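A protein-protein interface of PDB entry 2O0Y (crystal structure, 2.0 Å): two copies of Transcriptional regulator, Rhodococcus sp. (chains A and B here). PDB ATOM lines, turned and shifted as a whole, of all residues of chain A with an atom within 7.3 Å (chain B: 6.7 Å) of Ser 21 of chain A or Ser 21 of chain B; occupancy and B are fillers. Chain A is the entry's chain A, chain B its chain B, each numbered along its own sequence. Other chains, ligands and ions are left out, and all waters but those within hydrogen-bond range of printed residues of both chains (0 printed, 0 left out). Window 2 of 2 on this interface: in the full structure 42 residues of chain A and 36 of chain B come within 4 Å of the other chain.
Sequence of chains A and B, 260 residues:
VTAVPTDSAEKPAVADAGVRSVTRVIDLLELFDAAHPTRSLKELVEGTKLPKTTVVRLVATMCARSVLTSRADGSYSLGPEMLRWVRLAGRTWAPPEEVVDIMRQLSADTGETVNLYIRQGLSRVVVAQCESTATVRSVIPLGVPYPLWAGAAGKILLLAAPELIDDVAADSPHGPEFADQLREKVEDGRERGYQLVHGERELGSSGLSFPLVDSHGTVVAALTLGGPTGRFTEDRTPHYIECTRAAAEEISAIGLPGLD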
ATOM      1  N   GLY A  18     -16.345   8.727  -6.875  1.00  0.00           N
ATOM      2  CA  GLY A  18     -16.867  10.068  -6.345  1.00  0.00           C
ATOM      3  C   GLY A  18     -17.307  10.967  -7.500  1.00  0.00           C
ATOM      4  O   GLY A  18     -17.872  10.470  -8.491  1.00  0.00           O
ATOM      5  N   VAL A  19     -17.080  12.289  -7.357  1.00  0.00           N
ATOM      6  CA  VAL A  19     -17.329  13.259  -8.440  1.00  0.00           C
ATOM      7  C   VAL A  19     -16.254  13.056  -9.516  1.00  0.00           C
ATOM      8  O   VAL A  19     -15.049  13.176  -9.245  1.00  0.00           O
ATOM      9  CB  VAL A  19     -17.409  14.751  -7.941  1.00  0.00           C
ATOM     10  CG1 VAL A  19     -17.841  15.680  -9.079  1.00  0.00           C
ATOM     11  CG2 VAL A  19     -18.399  14.881  -6.783  1.00  0.00           C
ATOM     12  N   ARG A  20     -16.729  12.725 -10.722  1.00  0.00           N
ATOM     13  CA  ARG A  20     -15.920  12.253 -11.841  1.00  0.00           C
ATOM     14  C   ARG A  20     -14.806  13.209 -12.205  1.00  0.00           C
ATOM     15  O   ARG A  20     -13.640  12.813 -12.250  1.00  0.00           O
ATOM     16  CB  ARG A  20     -16.820  12.051 -13.061  1.00  0.00           C
ATOM     17  CG  ARG A  20     -16.484  10.827 -13.934  1.00  0.00           C
ATOM     18  CD  ARG A  20     -17.575  10.609 -14.983  1.00  0.00           C
ATOM     19  NE  ARG A  20     -17.940  11.873 -15.637  1.00  0.00           N
ATOM     20  CZ  ARG A  20     -18.917  12.016 -16.529  1.00  0.00           C
ATOM     21  NH1 ARG A  20     -19.654  10.976 -16.900  1.00  0.00           N
ATOM     22  NH2 ARG A  20     -19.163  13.212 -17.047  1.00  0.00           N
ATOM     23  N   SER A  21     -15.125  14.483 -12.453  1.00  0.00           N
ATOM     24  CA  SER A  21     -14.051  15.407 -12.869  1.00  0.00           C
ATOM     25  C   SER A  21     -12.982  15.645 -11.809  1.00  0.00           C
ATOM     26  O   SER A  21     -11.820  15.848 -12.128  1.00  0.00           O
ATOM     27  CB  SER A  21     -14.578  16.723 -13.459  1.00  0.00           C
ATOM     28  OG  SER A  21     -15.574  17.289 -12.582  1.00  0.00           O
ATOM     29  N   VAL A  22     -13.365  15.575 -10.544  1.00  0.00           N
ATOM     30  CA  VAL A  22     -12.421  15.707  -9.431  1.00  0.00           C
ATOM     31  C   VAL A  22     -11.530  14.447  -9.290  1.00  0.00           C
ATOM     32  O   VAL A  22     -10.343  14.530  -9.024  1.00  0.00           O
ATOM     33  CB  VAL A  22     -13.199  15.912  -8.155  1.00  0.00           C
ATOM     34  CG1 VAL A  22     -12.244  15.945  -6.915  1.00  0.00           C
ATOM     35  CG2 VAL A  22     -13.989  17.168  -8.277  1.00  0.00           C
ATOM     36  N   THR A  23     -12.133  13.276  -9.464  1.00  0.00           N
ATOM     37  CA  THR A  23     -11.394  12.014  -9.551  1.00  0.00           C
ATOM     38  C   THR A  23     -10.322  12.093 -10.647  1.00  0.00           C
ATOM     39  O   THR A  23      -9.178  11.692 -10.459  1.00  0.00           O
ATOM     40  CB  THR A  23     -12.409  10.917  -9.807  1.00  0.00           C
ATOM     41  OG1 THR A  23     -13.108  10.696  -8.585  1.00  0.00           O
ATOM     42  CG2 THR A  23     -11.757   9.613 -10.333  1.00  0.00           C
ATOM     43  N   ARG A  24     -10.706  12.688 -11.773  1.00  0.00           N
ATOM     44  CA  ARG A  24      -9.854  12.815 -12.954  1.00  0.00           C
ATOM     45  C   ARG A  24      -8.706  13.799 -12.799  1.00  0.00           C
ATOM     46  O   ARG A  24      -7.592  13.523 -13.220  1.00  0.00           O
ATOM     47  CB  ARG A  24     -10.704  13.213 -14.174  1.00  0.00           C
ATOM     48  CG  ARG A  24     -11.695  12.144 -14.607  1.00  0.00           C
ATOM     49  CD  ARG A  24     -12.621  12.664 -15.699  1.00  0.00           C
ATOM     50  NE  ARG A  24     -13.536  11.625 -16.135  1.00  0.00           N
ATOM     51  CZ  ARG A  24     -14.428  11.769 -17.111  1.00  0.00           C
ATOM     52  NH1 ARG A  24     -14.532  12.924 -17.764  1.00  0.00           N
ATOM     53  NH2 ARG A  24     -15.225  10.754 -17.438  1.00  0.00           N
ATOM     54  N   VAL A  25      -8.957  14.953 -12.214  1.00  0.00           N
ATOM     55  CA  VAL A  25      -7.865  15.859 -11.975  1.00  0.00           C
ATOM     56  C   VAL A  25      -6.856  15.197 -11.037  1.00  0.00           C
ATOM     57  O   VAL A  25      -5.655  15.287 -11.261  1.00  0.00           O
ATOM     58  CB  VAL A  25      -8.388  17.201 -11.460  1.00  0.00           C
ATOM     59  CG1 VAL A  25      -7.309  18.045 -10.868  1.00  0.00           C
ATOM     60  CG2 VAL A  25      -8.975  17.921 -12.663  1.00  0.00           C
ATOM     61  N   ILE A  26      -7.339  14.551  -9.976  1.00  0.00           N
ATOM     62  CA  ILE A  26      -6.422  13.896  -9.027  1.00  0.00           C
ATOM     63  C   ILE A  26      -5.668  12.753  -9.726  1.00  0.00           C
ATOM     64  O   ILE A  26      -4.469  12.662  -9.603  1.00  0.00           O
ATOM     65  CB  ILE A  26      -7.154  13.400  -7.798  1.00  0.00           C
ATOM     66  CG1 ILE A  26      -7.752  14.589  -7.069  1.00  0.00           C
ATOM     67  CG2 ILE A  26      -6.179  12.717  -6.831  1.00  0.00           C
ATOM     68  CD1 ILE A  26      -8.859  14.210  -6.154  1.00  0.00           C
ATOM     69  N   ASP A  27      -6.381  11.902 -10.480  1.00  0.00           N
ATOM     70  CA  ASP A  27      -5.747  10.891 -11.323  1.00  0.00           C
ATOM     71  C   ASP A  27      -4.646  11.488 -12.175  1.00  0.00           C
ATOM     72  O   ASP A  27      -3.531  10.969 -12.201  1.00  0.00           O
ATOM     73  CB  ASP A  27      -6.776  10.191 -12.212  1.00  0.00           C
ATOM     74  CG  ASP A  27      -7.696   9.267 -11.427  1.00  0.00           C
ATOM     75  OD1 ASP A  27      -7.497   9.077 -10.207  1.00  0.00           O
ATOM     76  OD2 ASP A  27      -8.643   8.762 -12.034  1.00  0.00           O
ATOM     77  N   LEU A  58      -9.065  20.076 -19.151  1.00  0.00           N
ATOM     78  CA  LEU A  58      -8.588  19.976 -17.754  1.00  0.00           C
ATOM     79  C   LEU A  58      -7.186  20.573 -17.553  1.00  0.00           C
ATOM     80  O   LEU A  58      -6.925  21.249 -16.553  1.00  0.00           O
ATOM     81  CB  LEU A  58      -8.605  18.524 -17.236  1.00  0.00           C
ATOM     82  CG  LEU A  58      -9.954  17.772 -17.152  1.00  0.00           C
ATOM     83  CD1 LEU A  58      -9.830  16.369 -16.523  1.00  0.00           C
ATOM     84  CD2 LEU A  58     -11.051  18.563 -16.447  1.00  0.00           C
ATOM     85  N   ALA B  17     -18.484  22.202 -16.745  1.00  0.00           N
ATOM     86  CA  ALA B  17     -19.405  21.253 -16.011  1.00  0.00           C
ATOM     87  C   ALA B  17     -18.566  20.275 -15.199  1.00  0.00           C
ATOM     88  O   ALA B  17     -18.643  20.232 -13.952  1.00  0.00           O
ATOM     89  CB  ALA B  17     -20.287  20.505 -16.989  1.00  0.00           C
ATOM     90  N   GLY B  18     -17.769  19.487 -15.920  1.00  0.00           N
ATOM     91  CA  GLY B  18     -16.622  18.809 -15.347  1.00  0.00           C
ATOM     92  C   GLY B  18     -15.589  19.855 -14.964  1.00  0.00           C
ATOM     93  O   GLY B  18     -15.016  19.797 -13.872  1.00  0.00           O
ATOM     94  N   VAL B  19     -15.359  20.830 -15.847  1.00  0.00           N
ATOM     95  CA  VAL B  19     -14.427  21.938 -15.546  1.00  0.00           C
ATOM     96  C   VAL B  19     -14.923  22.824 -14.408  1.00  0.00           C
ATOM     97  O   VAL B  19     -14.114  23.416 -13.682  1.00  0.00           O
ATOM     98  CB  VAL B  19     -14.113  22.817 -16.794  1.00  0.00           C
ATOM     99  CG1 VAL B  19     -13.622  24.215 -16.406  1.00  0.00           C
ATOM    100  CG2 VAL B  19     -13.093  22.143 -17.690  1.00  0.00           C
ATOM    101  N   ARG B  20     -16.241  22.959 -14.269  1.00  0.00           N
ATOM    102  CA  ARG B  20     -16.802  23.752 -13.164  1.00  0.00           C
ATOM    103  C   ARG B  20     -16.439  23.112 -11.827  1.00  0.00           C
ATOM    104  O   ARG B  20     -16.032  23.807 -10.905  1.00  0.00           O
ATOM    105  CB  ARG B  20     -18.315  23.896 -13.295  1.00  0.00           C
ATOM    106  CG  ARG B  20     -18.882  25.058 -12.509  1.00  0.00           C
ATOM    107  N   SER B  21     -16.575  21.794 -11.720  1.00  0.00           N
ATOM    108  CA  SER B  21     -16.210  21.093 -10.489  1.00  0.00           C
ATOM    109  C   SER B  21     -14.755  21.215 -10.158  1.00  0.00           C
ATOM    110  O   SER B  21     -14.369  21.264  -8.973  1.00  0.00           O
ATOM    111  CB  SER B  21     -16.653  19.620 -10.517  1.00  0.00           C
ATOM    112  OG  SER B  21     -18.075  19.575 -10.353  1.00  0.00           O
ATOM    113  N   VAL B  22     -13.923  21.195 -11.191  1.00  0.00           N
ATOM    114  CA  VAL B  22     -12.484  21.251 -10.988  1.00  0.00           C
ATOM    115  C   VAL B  22     -12.106  22.656 -10.518  1.00  0.00           C
ATOM    116  O   VAL B  22     -11.300  22.762  -9.648  1.00  0.00           O
ATOM    117  CB  VAL B  22     -11.706  20.818 -12.260  1.00  0.00           C
ATOM    118  CG1 VAL B  22     -10.195  21.178 -12.174  1.00  0.00           C
ATOM    119  CG2 VAL B  22     -11.928  19.317 -12.511  1.00  0.00           C
ATOM    120  N   THR B  23     -12.691  23.719 -11.074  1.00  0.00           N
ATOM    121  CA  THR B  23     -12.494  25.095 -10.557  1.00  0.00           C
ATOM    122  C   THR B  23     -12.907  25.247  -9.093  1.00  0.00           C
ATOM    123  O   THR B  23     -12.281  25.976  -8.318  1.00  0.00           O
ATOM    124  CB  THR B  23     -13.373  26.059 -11.356  1.00  0.00           C
ATOM    125  OG1 THR B  23     -12.874  26.056 -12.670  1.00  0.00           O
ATOM    126  CG2 THR B  23     -13.234  27.481 -10.820  1.00  0.00           C
ATOM    127  N   ARG B  24     -14.014  24.594  -8.727  1.00  0.00           N
ATOM    128  CA  ARG B  24     -14.482  24.608  -7.375  1.00  0.00           C
ATOM    129  C   ARG B  24     -13.499  23.882  -6.462  1.00  0.00           C
ATOM    130  O   ARG B  24     -13.271  24.301  -5.354  1.00  0.00           O
ATOM    131  CB  ARG B  24     -15.872  23.937  -7.315  1.00  0.00           C
ATOM    132  CG  ARG B  24     -16.958  24.880  -7.984  1.00  0.00           C
ATOM    133  CD  ARG B  24     -18.234  24.126  -8.245  1.00  0.00           C
ATOM    134  NE  ARG B  24     -19.253  25.085  -8.684  1.00  0.00           N
ATOM    135  CZ  ARG B  24     -20.511  24.779  -8.942  1.00  0.00           C
ATOM    136  NH1 ARG B  24     -20.921  23.533  -8.796  1.00  0.00           N
ATOM    137  NH2 ARG B  24     -21.340  25.727  -9.329  1.00  0.00           N
ATOM    138  N   VAL B  25     -12.949  22.761  -6.894  1.00  0.00           N
ATOM    139  CA  VAL B  25     -11.948  22.077  -6.099  1.00  0.00           C
ATOM    140  C   VAL B  25     -10.728  22.974  -5.887  1.00  0.00           C
ATOM    141  O   VAL B  25     -10.221  23.104  -4.808  1.00  0.00           O
ATOM    142  CB  VAL B  25     -11.547  20.732  -6.774  1.00  0.00           C
ATOM    143  CG1 VAL B  25     -10.463  20.094  -6.007  1.00  0.00           C
ATOM    144  CG2 VAL B  25     -12.792  19.799  -6.773  1.00  0.00           C
ATOM    145  N   ILE B  26     -10.238  23.578  -6.947  1.00  0.00           N
ATOM    146  CA  ILE B  26      -9.158  24.571  -6.816  1.00  0.00           C
ATOM    147  C   ILE B  26      -9.549  25.733  -5.903  1.00  0.00           C
ATOM    148  O   ILE B  26      -8.745  26.148  -5.050  1.00  0.00           O
ATOM    149  CB  ILE B  26      -8.687  25.046  -8.225  1.00  0.00           C
ATOM    150  CG1 ILE B  26      -8.171  23.842  -9.034  1.00  0.00           C
ATOM    151  CG2 ILE B  26      -7.597  26.141  -8.112  1.00  0.00           C
ATOM    152  CD1 ILE B  26      -8.011  24.159 -10.590  1.00  0.00           C
ATOM    153  N   ARG B  57     -20.613  18.015  -0.818  1.00  0.00           N
ATOM    154  CA  ARG B  57     -20.326  16.963  -1.796  1.00  0.00           C
ATOM    155  C   ARG B  57     -18.851  16.957  -2.248  1.00  0.00           C
ATOM    156  O   ARG B  57     -18.216  15.905  -2.374  1.00  0.00           O
ATOM    157  CB  ARG B  57     -21.252  17.111  -2.994  1.00  0.00           C
ATOM    158  CG  ARG B  57     -20.841  16.343  -4.240  1.00  0.00           C
ATOM    159  CD  ARG B  57     -22.010  16.179  -5.255  1.00  0.00           C
ATOM    160  NE  ARG B  57     -22.739  17.423  -5.582  1.00  0.00           N
ATOM    161  CZ  ARG B  57     -22.225  18.581  -6.030  1.00  0.00           C
ATOM    162  NH1 ARG B  57     -20.905  18.765  -6.180  1.00  0.00           N
ATOM    163  NH2 ARG B  57     -23.056  19.598  -6.282  1.00  0.00           N
ATOM    164  N   LEU B  58     -18.307  18.135  -2.511  1.00  0.00           N
ATOM    165  CA  LEU B  58     -16.896  18.197  -2.981  1.00  0.00           C
ATOM    166  C   LEU B  58     -15.954  17.822  -1.877  1.00  0.00           C
ATOM    167  O   LEU B  58     -14.977  17.084  -2.124  1.00  0.00           O
ATOM    168  CB  LEU B  58     -16.540  19.584  -3.549  1.00  0.00           C
ATOM    169  CG  LEU B  58     -17.263  19.979  -4.845  1.00  0.00           C
ATOM    170  CD1 LEU B  58     -17.137  21.513  -5.167  1.00  0.00           C
ATOM    171  CD2 LEU B  58     -16.747  19.131  -6.034  1.00  0.00           C
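Ser 21 of chain B touches just one residue of chain A: Ser 21.
Printed residues of chain A within 4 Å of Gly 18 of chain B: Ser 21 (2.9 Å).
Of the printed residues of chain B, Val 25 of chain A touches Val 22.
Printed residues of chain A within 4 Å of Val 22 of chain B: Ser 21 (3.5 Å) and Val 25 (3.3 Å).
Of the printed residues of chain A, Arg 57 of chain B touches Val 19 (3.8 Å).
Of the printed residues of chain A, Val 25 of chain B touches Val 22.
Thr 23 of chain A touches none of the printed residues of chain B.
The nearest printed residue of chain A that does not touch Arg 57 of chain B is Gly 18 of chain A (7.2 Å).
Ser 21 of chain A touches Gly 18 of chain B, but with the chains exchanged Gly 18 of chain A does not touch Ser 21 of chain B (9.1 Å).
Ser 21 of chain A touches its own counterpart, Ser 21 of chain B.
Ser 21 of chain A touches Val 22 of chain B, but with the chains exchanged Val 22 of chain A does not touch Ser 21 of chain B (4.2 Å).
Val 22 of chain A touches Val 25 of chain B, and with the chains exchanged Val 25 of chain A touches Val 22 of chain B.
10 positions are printed for both chains.
Of the 6 pairs that touch across the chains among the printed residues, 3 have their exchanged pair printed and touching as well.
The backbone carbonyl oxygen of Val 19 of chain A lies within hydrogen-bond range of the side-chain hydroxyl of Thr 23 of chain A (3.2 Å).
Printed residues of chain A that touch a printed residue of chain B: Val 19, Ser 21, Val 22 and Val 25.
Of the 12 printed residues of chain B, 5 touch a printed residue of chain A.
Hydrophobic or aromatic side chains of chain B within 4 Å of the printed part of chain A: Val 22 and Val 25.
Among the printed residues, 6 pairs touch across the chains.
Among the printed residues, no Asp or Glu carboxylate lies within 4 Å of a Lys or Arg side-chain nitrogen of the other chain.
The side-chain hydroxyl of Ser 21 of chain A sits at hydrogen-bond distance from the backbone carbonyl oxygen of Gly 18 of chain B, 2.9 Å away.
Among the printed residues, merely in contact across the chains: Val 22 of chain A with Val 25 of chain B (3.3 Å), Val 25 of chain A with Val 22 of chain B (3.3 Å), Ser 21 of chain A with Ser 21 of chain B (3.3 Å), Ser 21 of chain A with Val 22 of chain B (3.5 Å) and Val 19 of chain A with Arg 57 of chain B (3.8 Å).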
